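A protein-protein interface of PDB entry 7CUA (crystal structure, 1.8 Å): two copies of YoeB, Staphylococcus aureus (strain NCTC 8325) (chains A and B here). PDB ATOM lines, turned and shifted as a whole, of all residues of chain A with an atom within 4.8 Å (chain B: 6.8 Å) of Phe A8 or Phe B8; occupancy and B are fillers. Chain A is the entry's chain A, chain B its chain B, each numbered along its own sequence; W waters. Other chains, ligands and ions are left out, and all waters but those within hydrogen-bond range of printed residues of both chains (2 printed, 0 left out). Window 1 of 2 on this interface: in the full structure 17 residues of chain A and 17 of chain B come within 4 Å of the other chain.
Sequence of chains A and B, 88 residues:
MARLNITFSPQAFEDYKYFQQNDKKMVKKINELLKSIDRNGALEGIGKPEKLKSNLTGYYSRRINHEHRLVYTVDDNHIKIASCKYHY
Water W2 lies within hydrogen-bond range of the backbone carbonyl oxygen of Leu B4, the backbone carbonyl oxygen of Phe A8 and the backbone NH of Ile B6. Water W1 lies within hydrogen-bond range of OD1 of Asn A5 (2.7 Å) and NZ of Lys B80 (3.0 Å).
Printed residues of chain B that touch a printed residue of chain A: Leu B4, Asn B5, Ile B6, Thr B7, Phe B8, Ser B9, Pro B10, Phe B13, Tyr B16, Asn B31 and Leu B34. Hydrophobic or aromatic side chains of chain B within 4 Å of the printed part of chain A: Phe B8, Pro B10, Phe B13, Tyr B16 and Leu B34. Among the printed residues, 22 pairs touch across the chains. Among the printed residues, no Asp or Glu carboxylate lies within 4 Å of a Lys or Arg side-chain nitrogen of the other chain.
The backbone carbonyl oxygen of Ile A6 sits at hydrogen-bond distance from the backbone NH of Phe B8, at 2.7 Å. The side-chain hydroxyl (OG1) of Thr A7 lies within hydrogen-bond range of the side-chain hydroxyl (OG1) of Thr B7, at 2.9 Å. The backbone carbonyl oxygen (O) of Ile B6 sits at hydrogen-bond distance from the backbone NH (N) of Phe A8.
Asn A5 touches Thr B7, and with the chains exchanged Thr A7 touches Asn B5. Asn A5 touches Phe B8, and with the chains exchanged Phe A8 touches Asn B5. Phe A8 touches Phe B13, but with the chains exchanged Phe A13 does not touch Phe B8 (4.2 Å). Phe A13 touches Leu B34, but with the chains exchanged Leu A34 does not touch Phe B13 (4.04 Å). 11 positions are printed for both chains. Of the 22 pairs that touch across the chains among the printed residues, 18 have their exchanged pair printed and touching as well.
Among the printed residues, pairs that only touch across the chains: Asn A5 with Pro B10 (3.2 Å), Asn A5 with Phe B8 (3.3 Å), Thr A7 with Ile B6 (3.3 Å), Ile A6 with Thr B7 (3.3 Å), Pro A10 with Asn B5 (3.4 Å), Phe A8 with Asn B5 (3.4 Å), Ser A9 with Asn B5 (3.5 Å), Asn A5 with Ser B9 (3.5 Å), Ile A6 with Ile B6 (3.5 Å), Tyr A16 with Phe B13 (3.6 Å), Phe A13 with Asn B31 (3.6 Å), Asn A5 with Thr B7 (3.7 Å), Tyr A16 with Tyr B16 (3.7 Å), Phe A13 with Tyr B16 (3.7 Å), Pro A10 with Leu B4 (3.7 Å), Thr A7 with Asn B5 (3.8 Å), Phe A8 with Phe B8 (3.9 Å), Phe A13 with Leu B34 (3.9 Å) and Phe A8 with Phe B13 (3.99 Å).
Of the printed residues of chain B, Phe A8 touches Asn B5 (3.4 Å), Ile B6 (2.7 Å), Phe B8 (3.9 Å) and Phe B13 (3.99 Å). Of the printed residues of chain A, Phe B8 touches Asn A5, Ile A6 and Phe A8. Printed residues of chain B within 4 Å of Ile A6: Ile B6, Thr B7 and Phe B8. Printed residues of chain A within 4 Å of Phe B13: Phe A8 (3.99 Å) and Tyr A16 (3.6 Å). Of the printed residues of chain A, Asn B31 touches Phe A13. Printed residues of chain A within 4 Å of Leu B4: Pro A10. Cys B84 touches none of the printed residues of chain A. Ile B81 touches none of the printed residues of chain A. The nearest printed residue of chain B that does not touch Phe A8 is Leu B4 (4.7 Å).
The side-chain hydroxyl (OG) of Ser A9 sits at hydrogen-bond distance from the backbone NH (N) of Ala A12, at 3.1 Å. The backbone carbonyl oxygen (O) of Asn B5 lies within hydrogen-bond range of the backbone NH (N) of Ile B79, at 2.8 Å. The backbone NH (N) of Thr B7 lies within hydrogen-bond range of the backbone carbonyl oxygen (O) of Ile B79 (2.7 Å). The backbone carbonyl oxygen (O) of Thr B7 sits at hydrogen-bond distance from the backbone NH (N) of Ile B81 (2.7 Å). N of Ala B12 lies within hydrogen-bond range of OG of Ser B9. The backbone carbonyl oxygen of Ile B81 is in hydrogen-bond range of the backbone NH of Ser B9, at 3.0 Å.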
ATOM      1  N   ASN A   5     -17.416 -13.200  15.315  1.00  0.00           N
ATOM      2  CA  ASN A   5     -17.707 -14.024  16.476  1.00  0.00           C
ATOM      3  C   ASN A   5     -19.021 -13.569  17.110  1.00  0.00           C
ATOM      4  O   ASN A   5     -19.451 -12.426  16.948  1.00  0.00           O
ATOM      5  CB  ASN A   5     -16.576 -13.927  17.502  1.00  0.00           C
ATOM      6  CG  ASN A   5     -15.228 -14.360  16.939  1.00  0.00           C
ATOM      7  OD1 ASN A   5     -15.144 -15.269  16.103  1.00  0.00           O
ATOM      8  ND2 ASN A   5     -14.162 -13.712  17.403  1.00  0.00           N
ATOM      9  N   ILE A   6     -19.655 -14.476  17.851  1.00  0.00           N
ATOM     10  CA  ILE A   6     -20.879 -14.175  18.592  1.00  0.00           C
ATOM     11  C   ILE A   6     -20.578 -14.305  20.077  1.00  0.00           C
ATOM     12  O   ILE A   6     -20.270 -15.401  20.555  1.00  0.00           O
ATOM     13  CB  ILE A   6     -22.036 -15.102  18.194  1.00  0.00           C
ATOM     14  CG1 ILE A   6     -22.306 -15.019  16.689  1.00  0.00           C
ATOM     15  CG2 ILE A   6     -23.284 -14.745  18.993  1.00  0.00           C
ATOM     16  CD1 ILE A   6     -22.620 -13.627  16.206  1.00  0.00           C
ATOM     17  N   THR A   7     -20.670 -13.194  20.808  1.00  0.00           N
ATOM     18  CA  THR A   7     -20.331 -13.156  22.226  1.00  0.00           C
ATOM     19  C   THR A   7     -21.596 -12.911  23.039  1.00  0.00           C
ATOM     20  O   THR A   7     -22.277 -11.898  22.845  1.00  0.00           O
ATOM     21  CB  THR A   7     -19.295 -12.068  22.519  1.00  0.00           C
ATOM     22  OG1 THR A   7     -18.065 -12.383  21.853  1.00  0.00           O
ATOM     23  CG2 THR A   7     -19.032 -11.969  24.017  1.00  0.00           C
ATOM     24  N   PHE A   8     -21.899 -13.834  23.946  1.00  0.00           N
ATOM     25  CA  PHE A   8     -23.023 -13.713  24.862  1.00  0.00           C
ATOM     26  C   PHE A   8     -22.510 -13.262  26.222  1.00  0.00           C
ATOM     27  O   PHE A   8     -21.661 -13.933  26.821  1.00  0.00           O
ATOM     28  CB  PHE A   8     -23.757 -15.043  25.029  1.00  0.00           C
ATOM     29  CG  PHE A   8     -24.544 -15.480  23.832  1.00  0.00           C
ATOM     30  CD1 PHE A   8     -23.937 -16.203  22.814  1.00  0.00           C
ATOM     31  CD2 PHE A   8     -25.908 -15.225  23.754  1.00  0.00           C
ATOM     32  CE1 PHE A   8     -24.663 -16.628  21.720  1.00  0.00           C
ATOM     33  CE2 PHE A   8     -26.644 -15.653  22.664  1.00  0.00           C
ATOM     34  CZ  PHE A   8     -26.017 -16.357  21.645  1.00  0.00           C
ATOM     35  N   SER A   9     -23.037 -12.145  26.721  1.00  0.00           N
ATOM     36  CA  SER A   9     -22.841 -11.824  28.121  1.00  0.00           C
ATOM     37  C   SER A   9     -23.518 -12.896  28.973  1.00  0.00           C
ATOM     38  O   SER A   9     -24.366 -13.641  28.477  1.00  0.00           O
ATOM     39  CB  SER A   9     -23.427 -10.451  28.439  1.00  0.00           C
ATOM     40  OG  SER A   9     -24.839 -10.514  28.404  1.00  0.00           O
ATOM     41  N   PRO A  10     -23.155 -13.004  30.254  1.00  0.00           N
ATOM     42  CA  PRO A  10     -23.826 -13.998  31.109  1.00  0.00           C
ATOM     43  C   PRO A  10     -25.340 -13.872  31.117  1.00  0.00           C
ATOM     44  O   PRO A  10     -26.037 -14.888  31.012  1.00  0.00           O
ATOM     45  CB  PRO A  10     -23.221 -13.723  32.490  1.00  0.00           C
ATOM     46  CG  PRO A  10     -21.829 -13.239  32.172  1.00  0.00           C
ATOM     47  CD  PRO A  10     -21.988 -12.398  30.925  1.00  0.00           C
ATOM     48  N   ALA A  12     -27.188 -12.527  28.748  1.00  0.00           N
ATOM     49  CA  ALA A  12     -27.703 -12.819  27.414  1.00  0.00           C
ATOM     50  C   ALA A  12     -27.757 -14.317  27.161  1.00  0.00           C
ATOM     51  O   ALA A  12     -28.713 -14.817  26.557  1.00  0.00           O
ATOM     52  CB  ALA A  12     -26.843 -12.131  26.354  1.00  0.00           C
ATOM     53  N   PHE A  13     -26.738 -15.051  27.607  1.00  0.00           N
ATOM     54  CA  PHE A  13     -26.745 -16.496  27.412  1.00  0.00           C
ATOM     55  C   PHE A  13     -27.820 -17.149  28.265  1.00  0.00           C
ATOM     56  O   PHE A  13     -28.457 -18.118  27.836  1.00  0.00           O
ATOM     57  CB  PHE A  13     -25.369 -17.077  27.730  1.00  0.00           C
ATOM     58  CG  PHE A  13     -25.143 -18.444  27.152  1.00  0.00           C
ATOM     59  CD1 PHE A  13     -25.330 -18.678  25.800  1.00  0.00           C
ATOM     60  CD2 PHE A  13     -24.731 -19.492  27.960  1.00  0.00           C
ATOM     61  CE1 PHE A  13     -25.112 -19.937  25.263  1.00  0.00           C
ATOM     62  CE2 PHE A  13     -24.515 -20.751  27.430  1.00  0.00           C
ATOM     63  CZ  PHE A  13     -24.705 -20.972  26.081  1.00  0.00           C
ATOM     64  N   TYR A  16     -30.889 -16.632  26.338  1.00  0.00           N
ATOM     65  CA  TYR A  16     -30.898 -17.485  25.153  1.00  0.00           C
ATOM     66  C   TYR A  16     -31.256 -18.921  25.515  1.00  0.00           C
ATOM     67  O   TYR A  16     -32.062 -19.563  24.828  1.00  0.00           O
ATOM     68  CB  TYR A  16     -29.525 -17.399  24.483  1.00  0.00           C
ATOM     69  CG  TYR A  16     -29.388 -17.979  23.090  1.00  0.00           C
ATOM     70  CD1 TYR A  16     -29.981 -17.366  21.990  1.00  0.00           C
ATOM     71  CD2 TYR A  16     -28.606 -19.104  22.867  1.00  0.00           C
ATOM     72  CE1 TYR A  16     -29.830 -17.890  20.709  1.00  0.00           C
ATOM     73  CE2 TYR A  16     -28.444 -19.633  21.596  1.00  0.00           C
ATOM     74  CZ  TYR A  16     -29.056 -19.021  20.522  1.00  0.00           C
ATOM     75  OH  TYR A  16     -28.890 -19.554  19.265  1.00  0.00           O
ATOM     76  N   LEU A  34     -29.075 -12.138  14.294  1.00  0.00           N
ATOM     77  CA  LEU A  34     -27.617 -12.116  14.332  1.00  0.00           C
ATOM     78  C   LEU A  34     -27.030 -12.254  12.935  1.00  0.00           C
ATOM     79  O   LEU A  34     -26.021 -11.613  12.611  1.00  0.00           O
ATOM     80  CB  LEU A  34     -27.100 -13.227  15.245  1.00  0.00           C
ATOM     81  CG  LEU A  34     -27.440 -13.051  16.724  1.00  0.00           C
ATOM     82  CD1 LEU A  34     -27.105 -14.319  17.485  1.00  0.00           C
ATOM     83  CD2 LEU A  34     -26.691 -11.851  17.304  1.00  0.00           C
ATOM     84  N   ILE A  81     -23.652  -9.489  22.781  1.00  0.00           N
ATOM     85  CA  ILE A  81     -25.069  -9.450  23.129  1.00  0.00           C
ATOM     86  C   ILE A  81     -25.185  -9.223  24.626  1.00  0.00           C
ATOM     87  O   ILE A  81     -24.646 -10.002  25.422  1.00  0.00           O
ATOM     88  CB  ILE A  81     -25.784 -10.748  22.729  1.00  0.00           C
ATOM     89  CG1 ILE A  81     -25.519 -11.090  21.264  1.00  0.00           C
ATOM     90  CG2 ILE A  81     -27.268 -10.635  22.998  1.00  0.00           C
ATOM     91  CD1 ILE A  81     -25.912 -12.511  20.907  1.00  0.00           C
ATOM     92  N   LEU B   4     -18.223 -15.398  33.138  1.00  0.00           N
ATOM     93  CA  LEU B   4     -17.489 -15.132  31.908  1.00  0.00           C
ATOM     94  C   LEU B   4     -18.425 -14.990  30.714  1.00  0.00           C
ATOM     95  O   LEU B   4     -19.456 -15.661  30.624  1.00  0.00           O
ATOM     96  CB  LEU B   4     -16.487 -16.256  31.624  1.00  0.00           C
ATOM     97  CG  LEU B   4     -15.373 -16.472  32.649  1.00  0.00           C
ATOM     98  CD1 LEU B   4     -14.450 -17.593  32.181  1.00  0.00           C
ATOM     99  CD2 LEU B   4     -14.595 -15.186  32.880  1.00  0.00           C
ATOM    100  N   ASN B   5     -18.052 -14.106  29.790  1.00  0.00           N
ATOM    101  CA  ASN B   5     -18.714 -14.071  28.494  1.00  0.00           C
ATOM    102  C   ASN B   5     -18.475 -15.387  27.763  1.00  0.00           C
ATOM    103  O   ASN B   5     -17.474 -16.068  27.988  1.00  0.00           O
ATOM    104  CB  ASN B   5     -18.188 -12.911  27.648  1.00  0.00           C
ATOM    105  CG  ASN B   5     -18.460 -11.557  28.273  1.00  0.00           C
ATOM    106  OD1 ASN B   5     -19.471 -11.365  28.948  1.00  0.00           O
ATOM    107  ND2 ASN B   5     -17.554 -10.609  28.053  1.00  0.00           N
ATOM    108  N   ILE B   6     -19.401 -15.739  26.875  1.00  0.00           N
ATOM    109  CA  ILE B   6     -19.273 -16.928  26.030  1.00  0.00           C
ATOM    110  C   ILE B   6     -19.177 -16.463  24.586  1.00  0.00           C
ATOM    111  O   ILE B   6     -20.130 -15.873  24.061  1.00  0.00           O
ATOM    112  CB  ILE B   6     -20.455 -17.896  26.200  1.00  0.00           C
ATOM    113  CG1 ILE B   6     -20.599 -18.332  27.656  1.00  0.00           C
ATOM    114  CG2 ILE B   6     -20.264 -19.117  25.297  1.00  0.00           C
ATOM    115  CD1 ILE B   6     -19.496 -19.232  28.114  1.00  0.00           C
ATOM    116  N   THR B   7     -18.045 -16.738  23.939  1.00  0.00           N
ATOM    117  CA  THR B   7     -17.807 -16.307  22.566  1.00  0.00           C
ATOM    118  C   THR B   7     -17.749 -17.521  21.650  1.00  0.00           C
ATOM    119  O   THR B   7     -16.911 -18.411  21.846  1.00  0.00           O
ATOM    120  CB  THR B   7     -16.512 -15.499  22.454  1.00  0.00           C
ATOM    121  OG1 THR B   7     -16.590 -14.349  23.302  1.00  0.00           O
ATOM    122  CG2 THR B   7     -16.304 -15.036  21.019  1.00  0.00           C
ATOM    123  N   PHE B   8     -18.629 -17.551  20.650  1.00  0.00           N
ATOM    124  CA  PHE B   8     -18.602 -18.565  19.602  1.00  0.00           C
ATOM    125  C   PHE B   8     -17.854 -18.024  18.392  1.00  0.00           C
ATOM    126  O   PHE B   8     -18.141 -16.915  17.927  1.00  0.00           O
ATOM    127  CB  PHE B   8     -20.016 -18.962  19.166  1.00  0.00           C
ATOM    128  CG  PHE B   8     -20.811 -19.701  20.204  1.00  0.00           C
ATOM    129  CD1 PHE B   8     -21.529 -19.014  21.172  1.00  0.00           C
ATOM    130  CD2 PHE B   8     -20.877 -21.080  20.186  1.00  0.00           C
ATOM    131  CE1 PHE B   8     -22.283 -19.699  22.115  1.00  0.00           C
ATOM    132  CE2 PHE B   8     -21.632 -21.770  21.122  1.00  0.00           C
ATOM    133  CZ  PHE B   8     -22.332 -21.079  22.088  1.00  0.00           C
ATOM    134  N   SER B   9     -16.908 -18.807  17.873  1.00  0.00           N
ATOM    135  CA  SER B   9     -16.409 -18.544  16.534  1.00  0.00           C
ATOM    136  C   SER B   9     -17.547 -18.739  15.533  1.00  0.00           C
ATOM    137  O   SER B   9     -18.547 -19.389  15.843  1.00  0.00           O
ATOM    138  CB  SER B   9     -15.252 -19.482  16.196  1.00  0.00           C
ATOM    139  OG  SER B   9     -15.740 -20.775  15.873  1.00  0.00           O
ATOM    140  N   PRO B  10     -17.417 -18.190  14.320  1.00  0.00           N
ATOM    141  CA  PRO B  10     -18.449 -18.438  13.298  1.00  0.00           C
ATOM    142  C   PRO B  10     -18.751 -19.911  13.074  1.00  0.00           C
ATOM    143  O   PRO B  10     -19.929 -20.297  13.028  1.00  0.00           O
ATOM    144  CB  PRO B  10     -17.853 -17.772  12.052  1.00  0.00           C
ATOM    145  CG  PRO B  10     -17.044 -16.655  12.599  1.00  0.00           C
ATOM    146  CD  PRO B  10     -16.444 -17.177  13.876  1.00  0.00           C
ATOM    147  N   GLN B  11     -17.720 -20.752  12.947  1.00  0.00           N
ATOM    148  CA  GLN B  11     -17.968 -22.175  12.742  1.00  0.00           C
ATOM    149  C   GLN B  11     -18.619 -22.802  13.967  1.00  0.00           C
ATOM    150  O   GLN B  11     -19.548 -23.607  13.838  1.00  0.00           O
ATOM    151  CB  GLN B  11     -16.672 -22.908  12.403  1.00  0.00           C
ATOM    152  CG  GLN B  11     -16.910 -24.362  12.010  1.00  0.00           C
ATOM    153  CD  GLN B  11     -17.852 -24.477  10.829  1.00  0.00           C
ATOM    154  OE1 GLN B  11     -17.658 -23.815   9.810  1.00  0.00           O
ATOM    155  NE2 GLN B  11     -18.889 -25.306  10.963  1.00  0.00           N
ATOM    156  N   ALA B  12     -18.155 -22.433  15.163  1.00  0.00           N
ATOM    157  CA  ALA B  12     -18.711 -23.018  16.376  1.00  0.00           C
ATOM    158  C   ALA B  12     -20.188 -22.680  16.519  1.00  0.00           C
ATOM    159  O   ALA B  12     -20.990 -23.531  16.918  1.00  0.00           O
ATOM    160  CB  ALA B  12     -17.927 -22.544  17.599  1.00  0.00           C
ATOM    161  N   PHE B  13     -20.572 -21.444  16.192  1.00  0.00           N
ATOM    162  CA  PHE B  13     -21.979 -21.083  16.311  1.00  0.00           C
ATOM    163  C   PHE B  13     -22.821 -21.801  15.260  1.00  0.00           C
ATOM    164  O   PHE B  13     -23.964 -22.186  15.538  1.00  0.00           O
ATOM    165  CB  PHE B  13     -22.148 -19.567  16.215  1.00  0.00           C
ATOM    166  CG  PHE B  13     -23.485 -19.079  16.710  1.00  0.00           C
ATOM    167  CD1 PHE B  13     -23.892 -19.341  18.011  1.00  0.00           C
ATOM    168  CD2 PHE B  13     -24.336 -18.370  15.878  1.00  0.00           C
ATOM    169  CE1 PHE B  13     -25.127 -18.899  18.473  1.00  0.00           C
ATOM    170  CE2 PHE B  13     -25.576 -17.926  16.335  1.00  0.00           C
ATOM    171  CZ  PHE B  13     -25.965 -18.192  17.633  1.00  0.00           C
ATOM    172  N   GLU B  14     -22.271 -22.020  14.063  1.00  0.00           N
ATOM    173  CA  GLU B  14     -22.988 -22.831  13.086  1.00  0.00           C
ATOM    174  C   GLU B  14     -23.156 -24.262  13.584  1.00  0.00           C
ATOM    175  O   GLU B  14     -24.240 -24.841  13.457  1.00  0.00           O
ATOM    176  CB  GLU B  14     -22.274 -22.804  11.733  1.00  0.00           C
ATOM    177  CG  GLU B  14     -22.366 -21.463  11.000  1.00  0.00           C
ATOM    178  CD  GLU B  14     -23.797 -20.948  10.844  1.00  0.00           C
ATOM    179  OE1 GLU B  14     -24.024 -19.740  11.085  1.00  0.00           O
ATOM    180  OE2 GLU B  14     -24.691 -21.743  10.476  1.00  0.00           O
ATOM    181  N   TYR B  16     -23.333 -25.123  16.706  1.00  0.00           N
ATOM    182  CA  TYR B  16     -24.297 -25.022  17.794  1.00  0.00           C
ATOM    183  C   TYR B  16     -25.720 -24.916  17.262  1.00  0.00           C
ATOM    184  O   TYR B  16     -26.634 -25.571  17.775  1.00  0.00           O
ATOM    185  CB  TYR B  16     -23.927 -23.810  18.653  1.00  0.00           C
ATOM    186  CG  TYR B  16     -24.609 -23.689  19.994  1.00  0.00           C
ATOM    187  CD1 TYR B  16     -24.378 -24.609  21.010  1.00  0.00           C
ATOM    188  CD2 TYR B  16     -25.446 -22.618  20.261  1.00  0.00           C
ATOM    189  CE1 TYR B  16     -24.992 -24.477  22.246  1.00  0.00           C
ATOM    190  CE2 TYR B  16     -26.058 -22.472  21.491  1.00  0.00           C
ATOM    191  CZ  TYR B  16     -25.831 -23.400  22.480  1.00  0.00           C
ATOM    192  OH  TYR B  16     -26.449 -23.244  23.702  1.00  0.00           O
ATOM    193  N   ILE B  30     -23.447 -29.401  25.689  1.00  0.00           N
ATOM    194  CA  ILE B  30     -22.557 -28.255  25.505  1.00  0.00           C
ATOM    195  C   ILE B  30     -22.808 -27.204  26.581  1.00  0.00           C
ATOM    196  O   ILE B  30     -21.867 -26.640  27.156  1.00  0.00           O
ATOM    197  CB  ILE B  30     -22.733 -27.670  24.092  1.00  0.00           C
ATOM    198  CG1 ILE B  30     -22.163 -28.636  23.044  1.00  0.00           C
ATOM    199  CG2 ILE B  30     -22.110 -26.277  24.002  1.00  0.00           C
ATOM    200  CD1 ILE B  30     -22.624 -28.359  21.625  1.00  0.00           C
ATOM    201  N   ASN B  31     -24.081 -26.929  26.875  1.00  0.00           N
ATOM    202  CA  ASN B  31     -24.394 -25.943  27.904  1.00  0.00           C
ATOM    203  C   ASN B  31     -23.886 -26.389  29.270  1.00  0.00           C
ATOM    204  O   ASN B  31     -23.399 -25.567  30.053  1.00  0.00           O
ATOM    205  CB  ASN B  31     -25.902 -25.677  27.950  1.00  0.00           C
ATOM    206  CG  ASN B  31     -26.409 -24.978  26.699  1.00  0.00           C
ATOM    207  OD1 ASN B  31     -25.626 -24.466  25.899  1.00  0.00           O
ATOM    208  ND2 ASN B  31     -27.726 -24.936  26.536  1.00  0.00           N
ATOM    209  N   LEU B  34     -20.123 -25.820  29.364  1.00  0.00           N
ATOM    210  CA  LEU B  34     -19.805 -24.405  29.531  1.00  0.00           C
ATOM    211  C   LEU B  34     -19.988 -23.959  30.976  1.00  0.00           C
ATOM    212  O   LEU B  34     -19.201 -23.157  31.488  1.00  0.00           O
ATOM    213  CB  LEU B  34     -20.662 -23.559  28.587  1.00  0.00           C
ATOM    214  CG  LEU B  34     -20.340 -23.710  27.097  1.00  0.00           C
ATOM    215  CD1 LEU B  34     -21.443 -23.116  26.240  1.00  0.00           C
ATOM    216  CD2 LEU B  34     -19.013 -23.046  26.774  1.00  0.00           C
ATOM    217  N   LEU B  70     -15.956 -30.370  22.402  1.00  0.00           N
ATOM    218  CA  LEU B  70     -15.962 -28.917  22.451  1.00  0.00           C
ATOM    219  C   LEU B  70     -14.532 -28.421  22.606  1.00  0.00           C
ATOM    220  O   LEU B  70     -13.827 -28.854  23.518  1.00  0.00           O
ATOM    221  CB  LEU B  70     -16.803 -28.452  23.635  1.00  0.00           C
ATOM    222  CG  LEU B  70     -17.020 -26.964  23.836  1.00  0.00           C
ATOM    223  CD1 LEU B  70     -18.060 -26.491  22.842  1.00  0.00           C
ATOM    224  CD2 LEU B  70     -17.463 -26.696  25.264  1.00  0.00           C
ATOM    225  N   ILE B  79     -14.973 -17.366  27.737  1.00  0.00           N
ATOM    226  CA  ILE B  79     -14.705 -18.647  27.099  1.00  0.00           C
ATOM    227  C   ILE B  79     -14.873 -18.442  25.601  1.00  0.00           C
ATOM    228  O   ILE B  79     -15.896 -17.911  25.150  1.00  0.00           O
ATOM    229  CB  ILE B  79     -15.660 -19.735  27.617  1.00  0.00           C
ATOM    230  CG1 ILE B  79     -15.550 -19.876  29.137  1.00  0.00           C
ATOM    231  CG2 ILE B  79     -15.396 -21.074  26.910  1.00  0.00           C
ATOM    232  CD1 ILE B  79     -16.692 -20.650  29.750  1.00  0.00           C
ATOM    233  N   LYS B  80     -13.861 -18.822  24.835  1.00  0.00           N
ATOM    234  CA  LYS B  80     -13.886 -18.713  23.382  1.00  0.00           C
ATOM    235  C   LYS B  80     -13.983 -20.118  22.810  1.00  0.00           C
ATOM    236  O   LYS B  80     -13.118 -20.953  23.073  1.00  0.00           O
ATOM    237  CB  LYS B  80     -12.636 -17.998  22.864  1.00  0.00           C
ATOM    238  CG  LYS B  80     -12.485 -18.032  21.352  1.00  0.00           C
ATOM    239  CD  LYS B  80     -13.607 -17.269  20.675  1.00  0.00           C
ATOM    240  CE  LYS B  80     -13.602 -17.494  19.167  1.00  0.00           C
ATOM    241  NZ  LYS B  80     -12.281 -17.166  18.547  1.00  0.00           N
ATOM    242  N   ILE B  81     -15.038 -20.377  22.041  1.00  0.00           N
ATOM    243  CA  ILE B  81     -15.323 -21.704  21.509  1.00  0.00           C
ATOM    244  C   ILE B  81     -14.906 -21.741  20.047  1.00  0.00           C
ATOM    245  O   ILE B  81     -15.430 -20.979  19.226  1.00  0.00           O
ATOM    246  CB  ILE B  81     -16.811 -22.056  21.654  1.00  0.00           C
ATOM    247  CG1 ILE B  81     -17.260 -21.921  23.105  1.00  0.00           C
ATOM    248  CG2 ILE B  81     -17.066 -23.454  21.149  1.00  0.00           C
ATOM    249  CD1 ILE B  81     -18.771 -21.916  23.257  1.00  0.00           C
ATOM    250  N   ALA B  82     -13.988 -22.643  19.708  1.00  0.00           N
ATOM    251  CA  ALA B  82     -13.555 -22.778  18.324  1.00  0.00           C
ATOM    252  C   ALA B  82     -14.352 -23.819  17.548  1.00  0.00           C
ATOM    253  O   ALA B  82     -14.462 -23.708  16.322  1.00  0.00           O
ATOM    254  CB  ALA B  82     -12.064 -23.130  18.259  1.00  0.00           C
ATOM    255  N   CYS B  84     -17.608 -27.182  17.974  1.00  0.00           N
ATOM    256  CA  CYS B  84     -18.482 -28.074  18.726  1.00  0.00           C
ATOM    257  C   CYS B  84     -18.544 -29.470  18.119  1.00  0.00           C
ATOM    258  O   CYS B  84     -19.396 -30.267  18.522  1.00  0.00           O
ATOM    259  CB  CYS B  84     -19.899 -27.491  18.826  1.00  0.00           C
ATOM    260  SG  CYS B  84     -19.985 -25.866  19.613  1.00  0.00           S
HETATM  261  O   HOH W   1     -13.037 -16.883  15.611  1.00  0.00           O
HETATM  262  O   HOH W   2     -21.721 -15.840  29.346  1.00  0.00           O
